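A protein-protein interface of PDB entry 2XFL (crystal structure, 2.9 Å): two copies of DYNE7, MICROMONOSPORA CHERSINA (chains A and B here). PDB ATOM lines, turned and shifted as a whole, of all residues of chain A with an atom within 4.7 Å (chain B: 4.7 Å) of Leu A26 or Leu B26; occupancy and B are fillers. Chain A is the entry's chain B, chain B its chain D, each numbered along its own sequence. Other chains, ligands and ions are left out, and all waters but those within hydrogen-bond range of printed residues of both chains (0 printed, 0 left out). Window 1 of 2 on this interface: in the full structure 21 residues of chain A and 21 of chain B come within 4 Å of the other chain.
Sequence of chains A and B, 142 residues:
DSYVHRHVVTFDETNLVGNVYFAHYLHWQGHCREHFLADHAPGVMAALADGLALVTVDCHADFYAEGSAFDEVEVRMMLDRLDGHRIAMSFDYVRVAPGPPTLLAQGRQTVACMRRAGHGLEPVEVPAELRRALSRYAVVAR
NE2 of His A27 is in hydrogen-bond range of NE2 of His B27 (2.9 Å). The backbone NH (N) of Cys A59 sits at hydrogen-bond distance from the backbone carbonyl oxygen (O) of Ala B61 (3.1 Å). N of Ala A61 is in hydrogen-bond range of O of Cys B59 (3.0 Å).
NE2 of Gln A29 lies within hydrogen-bond range of O of His A60, at 3.3 Å. NE2 of Gln B29 sits at hydrogen-bond distance from O of His B60.
Among the printed residues, merely in contact across the chains: His A60 with His B60 (3.1 Å), Leu A26 with Phe B22 (3.3 Å), Phe A22 with Leu B26 (3.3 Å), Cys A59 with His B60 (3.3 Å), His A60 with Cys B59 (3.4 Å), His A27 with Ala B23 (3.5 Å), Ala A23 with His B27 (3.6 Å), Leu A26 with Leu B26 (3.8 Å), Leu A26 with Cys B59 (3.8 Å), Cys A59 with Leu B26 (3.8 Å) and Phe A22 with Cys B59 (3.9 Å).
Of the printed residues of chain B, Phe A22 touches Leu B26 (3.3 Å) and Cys B59 (3.9 Å). Of the printed residues of chain B, Leu A26 touches Phe B22, Leu B26 and Cys B59. Trp A28 touches none of the printed residues of chain B. Leu B26 touches just these residues of chain A: Phe A22 (3.3 Å), Leu A26 (3.8 Å) and Cys A59 (3.8 Å). Trp B28 touches none of the printed residues of chain A. Of the printed residues of chain A, His B60 touches Cys A59 (3.3 Å) and His A60 (3.1 Å). Of the printed residues of chain A, Ala B61 touches Cys A59 (3.1 Å). The nearest residue of chain B that does not touch Leu A26 is Ala B23 (4.2 Å). The nearest printed residue of chain B that does not touch Phe A22 is Gly B30 (4.04 Å).
Of the 12 printed residues of chain B, 7 touch a printed residue of chain A. Hydrophobic or aromatic side chains of chain B that line the printed part of chain A: Phe B22, Ala B23, Leu B26, His B27, His B60 and Ala B61. Along chain B the printed residues that touch a printed residue of chain A span positions 22 to 61. Hydrophobic or aromatic side chains of chain A within 4 Å of the printed part of chain B: Phe A22, Ala A23, Leu A26, His A27 and His A60. Among the printed residues, no Asp or Glu carboxylate lies within 4 Å of a Lys or Arg side-chain nitrogen of the other chain.
Phe A22 touches Leu B26, and with the chains exchanged Leu A26 touches Phe B22. Leu A26 touches Cys B59, and with the chains exchanged Cys A59 touches Leu B26. Cys A59 touches His B60, and with the chains exchanged His A60 touches Cys B59. His A60 touches its own counterpart, His B60. Positions printed for both chains: 22, 23, 24, 25, 26, 27, 28, 29, 30, 59, 60 and 61. Of the 14 pairs that touch across the chains among the printed residues, 13 have their exchanged pair printed and touching as well.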
ATOM      1  N   PHE A  22     -22.845 -10.436  -3.440  1.00  0.00           N
ATOM      2  CA  PHE A  22     -21.923  -9.552  -2.740  1.00  0.00           C
ATOM      3  C   PHE A  22     -20.448 -10.010  -2.733  1.00  0.00           C
ATOM      4  O   PHE A  22     -19.574  -9.209  -3.010  1.00  0.00           O
ATOM      5  CB  PHE A  22     -22.441  -9.179  -1.338  1.00  0.00           C
ATOM      6  CG  PHE A  22     -22.200 -10.205  -0.263  1.00  0.00           C
ATOM      7  CD1 PHE A  22     -23.091 -11.242  -0.065  1.00  0.00           C
ATOM      8  CD2 PHE A  22     -21.080 -10.131   0.547  1.00  0.00           C
ATOM      9  CE1 PHE A  22     -22.866 -12.185   0.925  1.00  0.00           C
ATOM     10  CE2 PHE A  22     -20.856 -11.066   1.540  1.00  0.00           C
ATOM     11  CZ  PHE A  22     -21.747 -12.090   1.721  1.00  0.00           C
ATOM     12  N   ALA A  23     -20.179 -11.292  -2.492  1.00  0.00           N
ATOM     13  CA  ALA A  23     -18.815 -11.784  -2.234  1.00  0.00           C
ATOM     14  C   ALA A  23     -17.893 -11.574  -3.396  1.00  0.00           C
ATOM     15  O   ALA A  23     -16.686 -11.444  -3.191  1.00  0.00           O
ATOM     16  CB  ALA A  23     -18.829 -13.258  -1.860  1.00  0.00           C
ATOM     17  N   HIS A  24     -18.404 -11.534  -4.710  1.00  0.00           N
ATOM     18  CA  HIS A  24     -17.641 -11.329  -5.943  1.00  0.00           C
ATOM     19  C   HIS A  24     -16.879 -10.043  -5.937  1.00  0.00           C
ATOM     20  O   HIS A  24     -15.779 -10.018  -6.470  1.00  0.00           O
ATOM     21  CB  HIS A  24     -18.551 -11.417  -7.144  1.00  0.00           C
ATOM     22  CG  HIS A  24     -19.080 -12.788  -7.299  1.00  0.00           C
ATOM     23  ND1 HIS A  24     -18.228 -13.879  -7.425  1.00  0.00           N
ATOM     24  CD2 HIS A  24     -20.352 -13.219  -7.273  1.00  0.00           C
ATOM     25  CE1 HIS A  24     -19.014 -14.928  -7.503  1.00  0.00           C
ATOM     26  NE2 HIS A  24     -20.302 -14.583  -7.409  1.00  0.00           N
ATOM     27  N   TYR A  25     -17.428  -8.977  -5.293  1.00  0.00           N
ATOM     28  CA  TYR A  25     -16.795  -7.668  -5.236  1.00  0.00           C
ATOM     29  C   TYR A  25     -15.442  -7.791  -4.518  1.00  0.00           C
ATOM     30  O   TYR A  25     -14.533  -7.030  -4.838  1.00  0.00           O
ATOM     31  CB  TYR A  25     -17.718  -6.655  -4.548  1.00  0.00           C
ATOM     32  CG  TYR A  25     -18.897  -6.174  -5.371  1.00  0.00           C
ATOM     33  CD1 TYR A  25     -18.867  -4.938  -6.021  1.00  0.00           C
ATOM     34  CD2 TYR A  25     -20.067  -6.921  -5.453  1.00  0.00           C
ATOM     35  CE1 TYR A  25     -19.973  -4.465  -6.746  1.00  0.00           C
ATOM     36  CE2 TYR A  25     -21.187  -6.451  -6.148  1.00  0.00           C
ATOM     37  CZ  TYR A  25     -21.144  -5.216  -6.786  1.00  0.00           C
ATOM     38  OH  TYR A  25     -22.256  -4.763  -7.477  1.00  0.00           O
ATOM     39  N   LEU A  26     -15.293  -8.781  -3.579  1.00  0.00           N
ATOM     40  CA  LEU A  26     -14.034  -9.041  -2.852  1.00  0.00           C
ATOM     41  C   LEU A  26     -12.965  -9.735  -3.721  1.00  0.00           C
ATOM     42  O   LEU A  26     -11.809  -9.297  -3.747  1.00  0.00           O
ATOM     43  CB  LEU A  26     -14.254  -9.757  -1.510  1.00  0.00           C
ATOM     44  CG  LEU A  26     -14.844  -8.919  -0.327  1.00  0.00           C
ATOM     45  CD1 LEU A  26     -14.169  -7.587  -0.152  1.00  0.00           C
ATOM     46  CD2 LEU A  26     -16.333  -8.674  -0.439  1.00  0.00           C
ATOM     47  N   HIS A  27     -13.369 -10.786  -4.473  1.00  0.00           N
ATOM     48  CA  HIS A  27     -12.563 -11.378  -5.562  1.00  0.00           C
ATOM     49  C   HIS A  27     -11.961 -10.311  -6.508  1.00  0.00           C
ATOM     50  O   HIS A  27     -10.777 -10.406  -6.848  1.00  0.00           O
ATOM     51  CB  HIS A  27     -13.403 -12.353  -6.390  1.00  0.00           C
ATOM     52  CG  HIS A  27     -13.738 -13.627  -5.679  1.00  0.00           C
ATOM     53  ND1 HIS A  27     -12.840 -14.687  -5.617  1.00  0.00           N
ATOM     54  CD2 HIS A  27     -14.881 -13.994  -5.077  1.00  0.00           C
ATOM     55  CE1 HIS A  27     -13.433 -15.620  -4.898  1.00  0.00           C
ATOM     56  NE2 HIS A  27     -14.666 -15.257  -4.565  1.00  0.00           N
ATOM     57  N   TRP A  28     -12.764  -9.301  -6.908  1.00  0.00           N
ATOM     58  CA  TRP A  28     -12.340  -8.269  -7.856  1.00  0.00           C
ATOM     59  C   TRP A  28     -11.216  -7.400  -7.310  1.00  0.00           C
ATOM     60  O   TRP A  28     -10.399  -6.939  -8.100  1.00  0.00           O
ATOM     61  CB  TRP A  28     -13.518  -7.394  -8.319  1.00  0.00           C
ATOM     62  CG  TRP A  28     -14.652  -8.139  -8.958  1.00  0.00           C
ATOM     63  CD1 TRP A  28     -14.636  -9.419  -9.432  1.00  0.00           C
ATOM     64  CD2 TRP A  28     -15.968  -7.625  -9.230  1.00  0.00           C
ATOM     65  NE1 TRP A  28     -15.870  -9.751  -9.948  1.00  0.00           N
ATOM     66  CE2 TRP A  28     -16.704  -8.666  -9.849  1.00  0.00           C
ATOM     67  CE3 TRP A  28     -16.592  -6.370  -9.033  1.00  0.00           C
ATOM     68  CZ2 TRP A  28     -18.044  -8.512 -10.237  1.00  0.00           C
ATOM     69  CZ3 TRP A  28     -17.917  -6.221  -9.431  1.00  0.00           C
ATOM     70  CH2 TRP A  28     -18.626  -7.282 -10.028  1.00  0.00           C
ATOM     71  N   GLN A  29     -11.179  -7.166  -5.964  1.00  0.00           N
ATOM     72  CA  GLN A  29     -10.087  -6.460  -5.249  1.00  0.00           C
ATOM     73  C   GLN A  29      -8.773  -7.241  -5.425  1.00  0.00           C
ATOM     74  O   GLN A  29      -7.711  -6.637  -5.578  1.00  0.00           O
ATOM     75  CB  GLN A  29     -10.378  -6.379  -3.749  1.00  0.00           C
ATOM     76  CG  GLN A  29     -11.478  -5.431  -3.362  1.00  0.00           C
ATOM     77  CD  GLN A  29     -11.632  -5.331  -1.870  1.00  0.00           C
ATOM     78  OE1 GLN A  29     -10.904  -5.961  -1.095  1.00  0.00           O
ATOM     79  NE2 GLN A  29     -12.596  -4.536  -1.438  1.00  0.00           N
ATOM     80  N   GLY A  30      -8.879  -8.564  -5.353  1.00  0.00           N
ATOM     81  CA  GLY A  30      -7.784  -9.484  -5.565  1.00  0.00           C
ATOM     82  C   GLY A  30      -7.274  -9.395  -6.969  1.00  0.00           C
ATOM     83  O   GLY A  30      -6.064  -9.308  -7.151  1.00  0.00           O
ATOM     84  N   CYS A  59     -10.475  -6.802   4.939  1.00  0.00           N
ATOM     85  CA  CYS A  59     -11.123  -6.227   3.787  1.00  0.00           C
ATOM     86  C   CYS A  59     -12.497  -5.729   4.172  1.00  0.00           C
ATOM     87  O   CYS A  59     -13.104  -6.237   5.099  1.00  0.00           O
ATOM     88  CB  CYS A  59     -11.194  -7.244   2.669  1.00  0.00           C
ATOM     89  SG  CYS A  59     -12.108  -8.742   3.095  1.00  0.00           S
ATOM     90  N   HIS A  60     -12.945  -4.838   3.405  1.00  0.00           N
ATOM     91  CA  HIS A  60     -14.260  -4.247   3.640  1.00  0.00           C
ATOM     92  C   HIS A  60     -14.854  -3.844   2.299  1.00  0.00           C
ATOM     93  O   HIS A  60     -14.107  -3.573   1.342  1.00  0.00           O
ATOM     94  CB  HIS A  60     -14.122  -3.031   4.548  1.00  0.00           C
ATOM     95  CG  HIS A  60     -15.423  -2.491   5.044  1.00  0.00           C
ATOM     96  ND1 HIS A  60     -16.131  -1.552   4.324  1.00  0.00           N
ATOM     97  CD2 HIS A  60     -16.106  -2.768   6.184  1.00  0.00           C
ATOM     98  CE1 HIS A  60     -17.221  -1.293   5.036  1.00  0.00           C
ATOM     99  NE2 HIS A  60     -17.259  -2.009   6.161  1.00  0.00           N
ATOM    100  N   ALA A  61     -16.196  -3.857   2.213  1.00  0.00           N
ATOM    101  CA  ALA A  61     -16.959  -3.412   1.038  1.00  0.00           C
ATOM    102  C   ALA A  61     -18.266  -2.721   1.483  1.00  0.00           C
ATOM    103  O   ALA A  61     -18.836  -3.099   2.504  1.00  0.00           O
ATOM    104  CB  ALA A  61     -17.251  -4.594   0.116  1.00  0.00           C
ATOM    105  N   PHE B  22      -8.664 -15.264   0.485  1.00  0.00           N
ATOM    106  CA  PHE B  22      -9.430 -14.396   1.398  1.00  0.00           C
ATOM    107  C   PHE B  22     -10.931 -14.310   1.062  1.00  0.00           C
ATOM    108  O   PHE B  22     -11.738 -14.439   1.972  1.00  0.00           O
ATOM    109  CB  PHE B  22      -8.769 -13.003   1.603  1.00  0.00           C
ATOM    110  CG  PHE B  22      -9.014 -12.028   0.483  1.00  0.00           C
ATOM    111  CD1 PHE B  22      -8.223 -12.053  -0.676  1.00  0.00           C
ATOM    112  CD2 PHE B  22     -10.060 -11.112   0.559  1.00  0.00           C
ATOM    113  CE1 PHE B  22      -8.473 -11.169  -1.735  1.00  0.00           C
ATOM    114  CE2 PHE B  22     -10.302 -10.225  -0.492  1.00  0.00           C
ATOM    115  CZ  PHE B  22      -9.508 -10.263  -1.636  1.00  0.00           C
ATOM    116  N   ALA B  23     -11.301 -14.193  -0.234  1.00  0.00           N
ATOM    117  CA  ALA B  23     -12.667 -13.864  -0.630  1.00  0.00           C
ATOM    118  C   ALA B  23     -13.674 -14.921  -0.233  1.00  0.00           C
ATOM    119  O   ALA B  23     -14.855 -14.613  -0.013  1.00  0.00           O
ATOM    120  CB  ALA B  23     -12.732 -13.600  -2.111  1.00  0.00           C
ATOM    121  N   HIS B  24     -13.197 -16.167  -0.075  1.00  0.00           N
ATOM    122  CA  HIS B  24     -13.999 -17.307   0.374  1.00  0.00           C
ATOM    123  C   HIS B  24     -14.657 -17.087   1.697  1.00  0.00           C
ATOM    124  O   HIS B  24     -15.798 -17.506   1.865  1.00  0.00           O
ATOM    125  CB  HIS B  24     -13.192 -18.597   0.335  1.00  0.00           C
ATOM    126  CG  HIS B  24     -12.810 -18.933  -1.066  1.00  0.00           C
ATOM    127  ND1 HIS B  24     -13.768 -19.127  -2.059  1.00  0.00           N
ATOM    128  CD2 HIS B  24     -11.594 -19.064  -1.619  1.00  0.00           C
ATOM    129  CE1 HIS B  24     -13.103 -19.399  -3.163  1.00  0.00           C
ATOM    130  NE2 HIS B  24     -11.794 -19.366  -2.959  1.00  0.00           N
ATOM    131  N   TYR B  25     -13.990 -16.411   2.601  1.00  0.00           N
ATOM    132  CA  TYR B  25     -14.519 -16.146   3.933  1.00  0.00           C
ATOM    133  C   TYR B  25     -15.822 -15.338   3.838  1.00  0.00           C
ATOM    134  O   TYR B  25     -16.692 -15.504   4.711  1.00  0.00           O
ATOM    135  CB  TYR B  25     -13.484 -15.427   4.827  1.00  0.00           C
ATOM    136  CG  TYR B  25     -12.337 -16.289   5.310  1.00  0.00           C
ATOM    137  CD1 TYR B  25     -12.335 -16.832   6.606  1.00  0.00           C
ATOM    138  CD2 TYR B  25     -11.239 -16.551   4.488  1.00  0.00           C
ATOM    139  CE1 TYR B  25     -11.262 -17.605   7.068  1.00  0.00           C
ATOM    140  CE2 TYR B  25     -10.166 -17.323   4.937  1.00  0.00           C
ATOM    141  CZ  TYR B  25     -10.172 -17.831   6.234  1.00  0.00           C
ATOM    142  OH  TYR B  25      -9.099 -18.577   6.671  1.00  0.00           O
ATOM    143  N   LEU B  26     -15.984 -14.527   2.758  1.00  0.00           N
ATOM    144  CA  LEU B  26     -17.182 -13.712   2.569  1.00  0.00           C
ATOM    145  C   LEU B  26     -18.349 -14.536   2.059  1.00  0.00           C
ATOM    146  O   LEU B  26     -19.463 -14.366   2.539  1.00  0.00           O
ATOM    147  CB  LEU B  26     -16.932 -12.467   1.710  1.00  0.00           C
ATOM    148  CG  LEU B  26     -16.192 -11.242   2.365  1.00  0.00           C
ATOM    149  CD1 LEU B  26     -16.818 -10.824   3.682  1.00  0.00           C
ATOM    150  CD2 LEU B  26     -14.669 -11.443   2.448  1.00  0.00           C
ATOM    151  N   HIS B  27     -18.099 -15.452   1.107  1.00  0.00           N
ATOM    152  CA  HIS B  27     -19.035 -16.508   0.664  1.00  0.00           C
ATOM    153  C   HIS B  27     -19.629 -17.249   1.859  1.00  0.00           C
ATOM    154  O   HIS B  27     -20.841 -17.473   1.894  1.00  0.00           O
ATOM    155  CB  HIS B  27     -18.333 -17.519  -0.258  1.00  0.00           C
ATOM    156  CG  HIS B  27     -18.051 -17.001  -1.624  1.00  0.00           C
ATOM    157  ND1 HIS B  27     -19.015 -16.991  -2.592  1.00  0.00           N
ATOM    158  CD2 HIS B  27     -16.924 -16.441  -2.124  1.00  0.00           C
ATOM    159  CE1 HIS B  27     -18.444 -16.465  -3.662  1.00  0.00           C
ATOM    160  NE2 HIS B  27     -17.199 -16.088  -3.417  1.00  0.00           N
ATOM    161  N   TRP B  28     -18.720 -17.608   2.952  1.00  0.00           N
ATOM    162  CA  TRP B  28     -19.142 -18.395   4.129  1.00  0.00           C
ATOM    163  C   TRP B  28     -20.144 -17.634   5.005  1.00  0.00           C
ATOM    164  O   TRP B  28     -20.993 -18.277   5.604  1.00  0.00           O
ATOM    165  CB  TRP B  28     -17.935 -18.892   4.963  1.00  0.00           C
ATOM    166  CG  TRP B  28     -16.924 -19.705   4.210  1.00  0.00           C
ATOM    167  CD1 TRP B  28     -17.080 -20.284   2.990  1.00  0.00           C
ATOM    168  CD2 TRP B  28     -15.598 -20.045   4.646  1.00  0.00           C
ATOM    169  NE1 TRP B  28     -15.920 -20.925   2.613  1.00  0.00           N
ATOM    170  CE2 TRP B  28     -15.004 -20.821   3.623  1.00  0.00           C
ATOM    171  CE3 TRP B  28     -14.855 -19.793   5.813  1.00  0.00           C
ATOM    172  CZ2 TRP B  28     -13.691 -21.312   3.713  1.00  0.00           C
ATOM    173  CZ3 TRP B  28     -13.557 -20.292   5.906  1.00  0.00           C
ATOM    174  CH2 TRP B  28     -12.993 -21.047   4.868  1.00  0.00           C
ATOM    175  N   GLN B  29     -20.035 -16.272   5.103  1.00  0.00           N
ATOM    176  CA  GLN B  29     -21.012 -15.391   5.781  1.00  0.00           C
ATOM    177  C   GLN B  29     -22.384 -15.510   5.137  1.00  0.00           C
ATOM    178  O   GLN B  29     -23.397 -15.478   5.829  1.00  0.00           O
ATOM    179  CB  GLN B  29     -20.605 -13.922   5.663  1.00  0.00           C
ATOM    180  CG  GLN B  29     -19.436 -13.536   6.476  1.00  0.00           C
ATOM    181  CD  GLN B  29     -19.192 -12.060   6.420  1.00  0.00           C
ATOM    182  OE1 GLN B  29     -19.902 -11.293   5.773  1.00  0.00           O
ATOM    183  NE2 GLN B  29     -18.171 -11.624   7.116  1.00  0.00           N
ATOM    184  N   GLY B  30     -22.476 -15.462   3.814  1.00  0.00           N
ATOM    185  CA  GLY B  30     -23.657 -15.668   2.990  1.00  0.00           C
ATOM    186  C   GLY B  30     -24.270 -17.015   3.272  1.00  0.00           C
ATOM    187  O   GLY B  30     -25.472 -17.080   3.506  1.00  0.00           O
ATOM    188  N   CYS B  59     -19.999  -5.388   4.165  1.00  0.00           N
ATOM    189  CA  CYS B  59     -19.416  -6.560   4.797  1.00  0.00           C
ATOM    190  C   CYS B  59     -17.961  -6.272   5.130  1.00  0.00           C
ATOM    191  O   CYS B  59     -17.320  -5.443   4.477  1.00  0.00           O
ATOM    192  CB  CYS B  59     -19.555  -7.791   3.912  1.00  0.00           C
ATOM    193  SG  CYS B  59     -18.639  -7.673   2.375  1.00  0.00           S
ATOM    194  N   HIS B  60     -17.450  -6.962   6.151  1.00  0.00           N
ATOM    195  CA  HIS B  60     -16.103  -6.821   6.646  1.00  0.00           C
ATOM    196  C   HIS B  60     -15.594  -8.169   7.109  1.00  0.00           C
ATOM    197  O   HIS B  60     -16.377  -8.982   7.572  1.00  0.00           O
ATOM    198  CB  HIS B  60     -16.067  -5.787   7.792  1.00  0.00           C
ATOM    199  CG  HIS B  60     -14.695  -5.360   8.164  1.00  0.00           C
ATOM    200  ND1 HIS B  60     -13.976  -6.051   9.101  1.00  0.00           N
ATOM    201  CD2 HIS B  60     -13.949  -4.332   7.707  1.00  0.00           C
ATOM    202  CE1 HIS B  60     -12.821  -5.414   9.214  1.00  0.00           C
ATOM    203  NE2 HIS B  60     -12.759  -4.371   8.393  1.00  0.00           N
ATOM    204  N   ALA B  61     -14.281  -8.401   6.976  1.00  0.00           N
ATOM    205  CA  ALA B  61     -13.551  -9.563   7.469  1.00  0.00           C
ATOM    206  C   ALA B  61     -12.136  -9.153   7.990  1.00  0.00           C
ATOM    207  O   ALA B  61     -11.527  -8.218   7.459  1.00  0.00           O
ATOM    208  CB  ALA B  61     -13.427 -10.590   6.371  1.00  0.00           C
